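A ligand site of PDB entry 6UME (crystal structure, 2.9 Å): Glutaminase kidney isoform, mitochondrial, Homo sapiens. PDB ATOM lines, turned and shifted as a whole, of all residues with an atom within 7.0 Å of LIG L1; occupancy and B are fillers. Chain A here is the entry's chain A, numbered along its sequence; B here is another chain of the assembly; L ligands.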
ATOM      1  N   ARG A 246      -2.335  14.279  30.640  1.00  0.00           N
ATOM      2  CA  ARG A 246      -2.250  15.721  30.727  1.00  0.00           C
ATOM      3  C   ARG A 246      -2.967  16.278  29.522  1.00  0.00           C
ATOM      4  O   ARG A 246      -3.196  17.494  29.436  1.00  0.00           O
ATOM      5  CB  ARG A 246      -0.788  16.186  30.816  1.00  0.00           C
ATOM      6  CG  ARG A 246      -0.471  17.283  31.823  1.00  0.00           C
ATOM      7  CD  ARG A 246       1.043  17.523  31.842  1.00  0.00           C
ATOM      8  NE  ARG A 246       1.654  16.445  32.601  1.00  0.00           N
ATOM      9  CZ  ARG A 246       2.918  16.424  32.993  1.00  0.00           C
ATOM     10  NH1 ARG A 246       3.395  15.376  33.664  1.00  0.00           N
ATOM     11  NH2 ARG A 246       3.686  17.468  32.758  1.00  0.00           N
ATOM     12  N   PHE A 247      -3.282  15.374  28.574  1.00  0.00           N
ATOM     13  CA  PHE A 247      -3.900  15.697  27.280  1.00  0.00           C
ATOM     14  C   PHE A 247      -5.307  15.242  27.150  1.00  0.00           C
ATOM     15  O   PHE A 247      -5.689  14.710  26.099  1.00  0.00           O
ATOM     16  CB  PHE A 247      -3.182  15.088  26.108  1.00  0.00           C
ATOM     17  CG  PHE A 247      -1.926  15.645  25.945  1.00  0.00           C
ATOM     18  CD1 PHE A 247      -1.640  16.734  26.730  1.00  0.00           C
ATOM     19  CD2 PHE A 247      -1.022  15.146  25.105  1.00  0.00           C
ATOM     20  CE1 PHE A 247      -0.498  17.254  26.764  1.00  0.00           C
ATOM     21  CE2 PHE A 247       0.121  15.735  25.048  1.00  0.00           C
ATOM     22  CZ  PHE A 247       0.385  16.774  25.933  1.00  0.00           C
ATOM     23  N   LYS A 249      -7.118  17.364  26.562  1.00  0.00           N
ATOM     24  CA  LYS A 249      -7.572  18.606  25.960  1.00  0.00           C
ATOM     25  C   LYS A 249      -6.940  18.970  24.615  1.00  0.00           C
ATOM     26  O   LYS A 249      -7.246  20.035  24.089  1.00  0.00           O
ATOM     27  CB  LYS A 249      -7.335  19.761  26.936  1.00  0.00           C
ATOM     28  CG  LYS A 249      -7.781  19.465  28.358  1.00  0.00           C
ATOM     29  CD  LYS A 249      -7.207  20.485  29.343  1.00  0.00           C
ATOM     30  CE  LYS A 249      -8.090  21.734  29.441  1.00  0.00           C
ATOM     31  NZ  LYS A 249      -7.578  22.715  30.434  1.00  0.00           N
ATOM     32  N   LEU A 250      -6.124  18.126  24.008  1.00  0.00           N
ATOM     33  CA  LEU A 250      -5.683  18.453  22.658  1.00  0.00           C
ATOM     34  C   LEU A 250      -6.590  17.786  21.639  1.00  0.00           C
ATOM     35  O   LEU A 250      -7.150  16.717  21.887  1.00  0.00           O
ATOM     36  CB  LEU A 250      -4.237  18.015  22.441  1.00  0.00           C
ATOM     37  CG  LEU A 250      -3.188  19.032  22.877  1.00  0.00           C
ATOM     38  CD1 LEU A 250      -3.147  19.229  24.413  1.00  0.00           C
ATOM     39  CD2 LEU A 250      -1.842  18.612  22.305  1.00  0.00           C
ATOM     40  N   PHE A 251      -6.737  18.422  20.472  1.00  0.00           N
ATOM     41  CA  PHE A 251      -7.703  17.886  19.524  1.00  0.00           C
ATOM     42  C   PHE A 251      -7.077  16.857  18.596  1.00  0.00           C
ATOM     43  O   PHE A 251      -7.735  15.884  18.234  1.00  0.00           O
ATOM     44  CB  PHE A 251      -8.331  18.988  18.648  1.00  0.00           C
ATOM     45  CG  PHE A 251      -9.263  19.919  19.385  1.00  0.00           C
ATOM     46  CD1 PHE A 251      -9.648  19.679  20.690  1.00  0.00           C
ATOM     47  CD2 PHE A 251      -9.744  21.053  18.765  1.00  0.00           C
ATOM     48  CE1 PHE A 251     -10.497  20.556  21.355  1.00  0.00           C
ATOM     49  CE2 PHE A 251     -10.592  21.919  19.420  1.00  0.00           C
ATOM     50  CZ  PHE A 251     -10.964  21.664  20.713  1.00  0.00           C
ATOM     51  N   LEU A 252      -5.813  17.061  18.236  1.00  0.00           N
ATOM     52  CA  LEU A 252      -5.145  16.246  17.235  1.00  0.00           C
ATOM     53  C   LEU A 252      -3.842  15.751  17.823  1.00  0.00           C
ATOM     54  O   LEU A 252      -3.167  16.480  18.547  1.00  0.00           O
ATOM     55  CB  LEU A 252      -4.861  17.063  15.955  1.00  0.00           C
ATOM     56  CG  LEU A 252      -6.081  17.658  15.267  1.00  0.00           C
ATOM     57  CD1 LEU A 252      -5.740  18.130  13.861  1.00  0.00           C
ATOM     58  CD2 LEU A 252      -7.150  16.596  15.218  1.00  0.00           C
ATOM     59  N   ASN A 253      -3.470  14.531  17.448  1.00  0.00           N
ATOM     60  CA  ASN A 253      -2.184  13.987  17.841  1.00  0.00           C
ATOM     61  C   ASN A 253      -1.115  14.525  16.881  1.00  0.00           C
ATOM     62  O   ASN A 253      -1.388  15.395  16.053  1.00  0.00           O
ATOM     63  CB  ASN A 253      -2.244  12.462  17.897  1.00  0.00           C
ATOM     64  CG  ASN A 253      -2.307  11.808  16.523  1.00  0.00           C
ATOM     65  OD1 ASN A 253      -2.147  12.459  15.483  1.00  0.00           O
ATOM     66  ND2 ASN A 253      -2.537  10.490  16.520  1.00  0.00           N
ATOM     67  N   GLU A 254       0.100  13.995  16.970  1.00  0.00           N
ATOM     68  CA  GLU A 254       1.206  14.624  16.243  1.00  0.00           C
ATOM     69  C   GLU A 254       1.131  14.419  14.737  1.00  0.00           C
ATOM     70  O   GLU A 254       1.765  15.187  13.998  1.00  0.00           O
ATOM     71  CB  GLU A 254       2.530  14.132  16.820  1.00  0.00           C
ATOM     72  CG  GLU A 254       3.024  15.072  17.914  1.00  0.00           C
ATOM     73  CD  GLU A 254       4.273  14.593  18.621  1.00  0.00           C
ATOM     74  OE1 GLU A 254       4.297  14.671  19.870  1.00  0.00           O
ATOM     75  OE2 GLU A 254       5.220  14.154  17.942  1.00  0.00           O
ATOM     76  N   ASP A 255       0.353  13.439  14.255  1.00  0.00           N
ATOM     77  CA  ASP A 255       0.142  13.256  12.821  1.00  0.00           C
ATOM     78  C   ASP A 255      -1.097  13.990  12.351  1.00  0.00           C
ATOM     79  O   ASP A 255      -1.603  13.698  11.272  1.00  0.00           O
ATOM     80  CB  ASP A 255       0.021  11.778  12.458  1.00  0.00           C
ATOM     81  CG  ASP A 255       1.154  10.911  13.022  1.00  0.00           C
ATOM     82  OD1 ASP A 255       2.326  11.346  12.962  1.00  0.00           O
ATOM     83  OD2 ASP A 255       0.878   9.794  13.510  1.00  0.00           O
ATOM     84  N   ASP A 256      -1.596  14.915  13.181  1.00  0.00           N
ATOM     85  CA  ASP A 256      -2.769  15.742  12.878  1.00  0.00           C
ATOM     86  C   ASP A 256      -4.038  14.917  12.657  1.00  0.00           C
ATOM     87  O   ASP A 256      -4.965  15.343  11.961  1.00  0.00           O
ATOM     88  CB  ASP A 256      -2.501  16.680  11.695  1.00  0.00           C
ATOM     89  CG  ASP A 256      -1.521  17.776  12.057  1.00  0.00           C
ATOM     90  OD1 ASP A 256      -1.716  18.427  13.110  1.00  0.00           O
ATOM     91  OD2 ASP A 256      -0.551  17.975  11.289  1.00  0.00           O
ATOM     92  N   HIS A 259      -6.829  11.593  18.370  1.00  0.00           N
ATOM     93  CA  HIS A 259      -6.027  10.548  19.007  1.00  0.00           C
ATOM     94  C   HIS A 259      -6.611   9.166  18.770  1.00  0.00           C
ATOM     95  O   HIS A 259      -5.865   8.202  18.537  1.00  0.00           O
ATOM     96  CB  HIS A 259      -5.878  10.831  20.494  1.00  0.00           C
ATOM     97  CG  HIS A 259      -5.251  12.149  20.777  1.00  0.00           C
ATOM     98  ND1 HIS A 259      -3.908  12.386  20.580  1.00  0.00           N
ATOM     99  CD2 HIS A 259      -5.774  13.322  21.218  1.00  0.00           C
ATOM    100  CE1 HIS A 259      -3.634  13.637  20.893  1.00  0.00           C
ATOM    101  NE2 HIS A 259      -4.749  14.228  21.282  1.00  0.00           N
ATOM    102  N   TYR A 323     -11.896  23.506  13.817  1.00  0.00           N
ATOM    103  CA  TYR A 323     -10.480  23.197  13.870  1.00  0.00           C
ATOM    104  C   TYR A 323     -10.145  22.031  12.960  1.00  0.00           C
ATOM    105  O   TYR A 323      -9.151  22.065  12.234  1.00  0.00           O
ATOM    106  CB  TYR A 323     -10.056  22.928  15.315  1.00  0.00           C
ATOM    107  CG  TYR A 323      -8.558  22.834  15.581  1.00  0.00           C
ATOM    108  CD1 TYR A 323      -7.802  23.951  15.911  1.00  0.00           C
ATOM    109  CD2 TYR A 323      -7.909  21.606  15.549  1.00  0.00           C
ATOM    110  CE1 TYR A 323      -6.427  23.834  16.195  1.00  0.00           C
ATOM    111  CE2 TYR A 323      -6.558  21.500  15.819  1.00  0.00           C
ATOM    112  CZ  TYR A 323      -5.825  22.606  16.139  1.00  0.00           C
ATOM    113  OH  TYR A 323      -4.486  22.439  16.402  1.00  0.00           O
ATOM    114  N   LYS A 327      -7.481  22.041   9.733  1.00  0.00           N
ATOM    115  CA  LYS A 327      -6.338  21.151   9.607  1.00  0.00           C
ATOM    116  C   LYS A 327      -6.608  19.974   8.686  1.00  0.00           C
ATOM    117  O   LYS A 327      -5.880  18.970   8.737  1.00  0.00           O
ATOM    118  CB  LYS A 327      -5.888  20.666  10.990  1.00  0.00           C
ATOM    119  CG  LYS A 327      -5.452  21.781  11.941  1.00  0.00           C
ATOM    120  CD  LYS A 327      -4.077  22.307  11.583  1.00  0.00           C
ATOM    121  CE  LYS A 327      -3.539  23.161  12.705  1.00  0.00           C
ATOM    122  NZ  LYS A 327      -3.207  22.323  13.892  1.00  0.00           N
ATOM    123  N   LEU B 245       2.087   9.759  24.019  1.00  0.00           N
ATOM    124  CA  LEU B 245       3.168  10.050  23.098  1.00  0.00           C
ATOM    125  C   LEU B 245       3.404  11.571  22.918  1.00  0.00           C
ATOM    126  O   LEU B 245       3.730  12.022  21.807  1.00  0.00           O
ATOM    127  CB  LEU B 245       2.925   9.364  21.748  1.00  0.00           C
ATOM    128  CG  LEU B 245       3.110   7.822  21.537  1.00  0.00           C
ATOM    129  CD1 LEU B 245       3.455   7.466  20.074  1.00  0.00           C
ATOM    130  CD2 LEU B 245       4.113   7.154  22.501  1.00  0.00           C
ATOM    131  N   ARG B 246       3.198  12.401  23.980  1.00  0.00           N
ATOM    132  CA  ARG B 246       3.937  13.649  24.232  1.00  0.00           C
ATOM    133  C   ARG B 246       4.907  13.432  25.385  1.00  0.00           C
ATOM    134  O   ARG B 246       6.027  13.953  25.374  1.00  0.00           O
ATOM    135  CB  ARG B 246       3.031  14.859  24.646  1.00  0.00           C
ATOM    136  CG  ARG B 246       3.646  16.420  24.742  1.00  0.00           C
ATOM    137  CD  ARG B 246       2.754  17.564  24.222  1.00  0.00           C
ATOM    138  NE  ARG B 246       2.930  18.895  24.836  1.00  0.00           N
ATOM    139  CZ  ARG B 246       2.017  19.865  24.670  1.00  0.00           C
ATOM    140  NH1 ARG B 246       0.895  19.606  24.082  1.00  0.00           N
ATOM    141  NH2 ARG B 246       2.110  21.051  25.207  1.00  0.00           N
HETATM  142  N1  LIG L   1      -7.696  23.892  23.276  1.00  0.00           N
HETATM  143  N2  LIG L   1      -5.123  20.688  19.702  1.00  0.00           N
HETATM  144  C1  LIG L   1      -6.364  22.354  21.863  1.00  0.00           C
HETATM  145  C2  LIG L   1      -6.351  23.212  20.582  1.00  0.00           C
HETATM  146  C3  LIG L   1      -4.567  21.917  19.561  1.00  0.00           C
HETATM  147  C4  LIG L   1      -3.145  19.898  18.890  1.00  0.00           C
HETATM  148  C5  LIG L   1      -0.833  19.288  18.144  1.00  0.00           C
HETATM  149  C6  LIG L   1       0.985  17.926  18.738  1.00  0.00           C
HETATM  150  C7  LIG L   1       2.624  17.217  20.853  1.00  0.00           C
HETATM  151  C8  LIG L   1      -6.878  24.365  24.374  1.00  0.00           C
HETATM  152  C9  LIG L   1      -5.747  24.796  29.113  1.00  0.00           C
HETATM  153  C10 LIG L   1      -3.096  23.275  30.879  1.00  0.00           C
HETATM  154  C11 LIG L   1      -1.722  23.035  30.806  1.00  0.00           C
HETATM  155  C12 LIG L   1      -0.879  24.028  30.288  1.00  0.00           C
HETATM  156  C13 LIG L   1      -6.481  24.556  21.190  1.00  0.00           C
HETATM  157  C14 LIG L   1       0.520  17.040  19.727  1.00  0.00           C
HETATM  158  C15 LIG L   1       1.342  16.673  20.782  1.00  0.00           C
HETATM  159  C16 LIG L   1       2.270  18.442  18.907  1.00  0.00           C
HETATM  160  C17 LIG L   1      -5.561  24.902  26.576  1.00  0.00           C
HETATM  161  C18 LIG L   1      -5.101  24.761  30.497  1.00  0.00           C
HETATM  162  C19 LIG L   1      -3.626  24.487  30.438  1.00  0.00           C
HETATM  163  C20 LIG L   1      -7.756  24.701  22.056  1.00  0.00           C
HETATM  164  C21 LIG L   1      -2.696  25.431  29.928  1.00  0.00           C
HETATM  165  C22 LIG L   1      -7.616  22.544  22.745  1.00  0.00           C
HETATM  166  C23 LIG L   1       0.162  18.339  17.640  1.00  0.00           C
HETATM  167  N3  LIG L   1      -1.368  25.222  29.848  1.00  0.00           N
HETATM  168  N4  LIG L   1      -5.130  23.104  19.852  1.00  0.00           N
HETATM  169  N5  LIG L   1      -4.377  19.643  19.345  1.00  0.00           N
HETATM  170  N6  LIG L   1      -2.188  18.954  18.410  1.00  0.00           N
HETATM  171  N7  LIG L   1       3.098  18.097  19.927  1.00  0.00           N
HETATM  172  N8  LIG L   1      -6.256  25.552  24.484  1.00  0.00           N
HETATM  173  N9  LIG L   1      -5.573  25.852  25.609  1.00  0.00           N
HETATM  174  N10 LIG L   1      -4.962  24.882  27.864  1.00  0.00           N
HETATM  175  O1  LIG L   1      -0.439  20.381  18.389  1.00  0.00           O
HETATM  176  O2  LIG L   1      -6.971  24.738  29.066  1.00  0.00           O
HETATM  177  S1  LIG L   1      -2.920  21.720  18.892  1.00  0.00           S
HETATM  178  S2  LIG L   1      -6.561  23.503  25.937  1.00  0.00           S
HETATM  179  N1  LG2 L   2      13.252  16.140  30.871  1.00  0.00           N
HETATM  180  N2  LG2 L   2       9.631  15.316  34.834  1.00  0.00           N
HETATM  181  C1  LG2 L   2      11.334  16.523  32.304  1.00  0.00           C
HETATM  182  C2  LG2 L   2      12.048  16.548  33.644  1.00  0.00           C
HETATM  183  C3  LG2 L   2       9.977  16.617  34.822  1.00  0.00           C
HETATM  184  C4  LG2 L   2       7.506  16.055  35.129  1.00  0.00           C
HETATM  185  C5  LG2 L   2       5.316  16.905  36.104  1.00  0.00           C
HETATM  186  C6  LG2 L   2       2.845  17.989  35.991  1.00  0.00           C
HETATM  187  C7  LG2 L   2       1.497  20.136  35.061  1.00  0.00           C
HETATM  188  C8  LG2 L   2      13.196  17.098  29.902  1.00  0.00           C
HETATM  189  C9  LG2 L   2      12.565  18.800  25.280  1.00  0.00           C
HETATM  190  C10 LG2 L   2      10.851  18.276  22.565  1.00  0.00           C
HETATM  191  C11 LG2 L   2       9.433  17.944  22.464  1.00  0.00           C
HETATM  192  C12 LG2 L   2       8.325  18.428  23.416  1.00  0.00           C
HETATM  193  C13 LG2 L   2      13.257  17.303  33.214  1.00  0.00           C
HETATM  194  C14 LG2 L   2       1.449  17.914  35.822  1.00  0.00           C
HETATM  195  C15 LG2 L   2       0.767  19.007  35.354  1.00  0.00           C
HETATM  196  C16 LG2 L   2       3.404  19.172  35.666  1.00  0.00           C
HETATM  197  C17 LG2 L   2      13.095  18.678  27.833  1.00  0.00           C
HETATM  198  C18 LG2 L   2      12.436  19.474  23.886  1.00  0.00           C
HETATM  199  C19 LG2 L   2      11.200  19.097  23.580  1.00  0.00           C
HETATM  200  C20 LG2 L   2      14.041  16.486  32.126  1.00  0.00           C
HETATM  201  C21 LG2 L   2      10.230  19.501  24.494  1.00  0.00           C
HETATM  202  C22 LG2 L   2      12.033  15.583  31.364  1.00  0.00           C
HETATM  203  C23 LG2 L   2       3.754  16.850  36.507  1.00  0.00           C
HETATM  204  N3  LG2 L   2       8.818  19.294  24.477  1.00  0.00           N
HETATM  205  N4  LG2 L   2      11.218  17.160  34.630  1.00  0.00           N
HETATM  206  N5  LG2 L   2       8.371  15.044  35.014  1.00  0.00           N
HETATM  207  N6  LG2 L   2       6.085  15.925  35.369  1.00  0.00           N
HETATM  208  N7  LG2 L   2       2.778  20.188  35.173  1.00  0.00           N
HETATM  209  N8  LG2 L   2      13.320  18.397  30.104  1.00  0.00           N
HETATM  210  N9  LG2 L   2      13.274  19.213  29.050  1.00  0.00           N
HETATM  211  N10 LG2 L   2      12.990  19.357  26.567  1.00  0.00           N
HETATM  212  O1  LG2 L   2       5.938  17.872  36.458  1.00  0.00           O
HETATM  213  O2  LG2 L   2      12.285  17.654  25.323  1.00  0.00           O
HETATM  214  S1  LG2 L   2       8.473  17.594  35.026  1.00  0.00           S
HETATM  215  S2  LG2 L   2      12.958  16.836  28.123  1.00  0.00           S
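NZ of Lys 327 is in hydrogen-bond range of OH of Tyr 323 (2.8 Å).
The side-chain amide oxygen (OD1) of Asn 253 is in hydrogen-bond range of the backbone NH (N) of Asp 256, at 3.4 Å.
The side-chain amide oxygen (OD1) of Asn 253 is in hydrogen-bond range of the backbone NH (N) of Asp 255 (3.0 Å).
Merely in contact with LIG L1: Glu 254, Arg 246 of chain B, Leu 250 and Asn 253.
Hydrophobic or aromatic side chains within 4 Å of LIG L1: Leu 250, Phe 251 and Tyr 323.
Eight residues have an atom within 4 Å of LIG L1: Lys 249, Leu 250, Phe 251, Leu 252, Asn 253, Glu 254, Tyr 323 and Arg 246 of chain B.
Along chain A the residues within 4 Å of LIG L1 span positions 249 to 323.
The nearest printed residue that does not touch LIG L1 is Phe 247 (4.5 Å).
An oxygen (O2) of LIG L1 lies within hydrogen-bond range of the side-chain amino group (NZ) of Lys 249, at 2.5 Å.
A nitrogen (N5) of LIG L1 sits at hydrogen-bond distance from the backbone NH (N) of Leu 252 (3.2 Å).
N6 of LIG L1 is in hydrogen-bond range of O of Leu 252 (2.7 Å).
N of Phe 251 is in hydrogen-bond range of N5 of LIG L1.
The side-chain hydroxyl (OH) of Tyr 323 lies close to a sulfur (S1) of LIG L1, at 3.0 Å.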
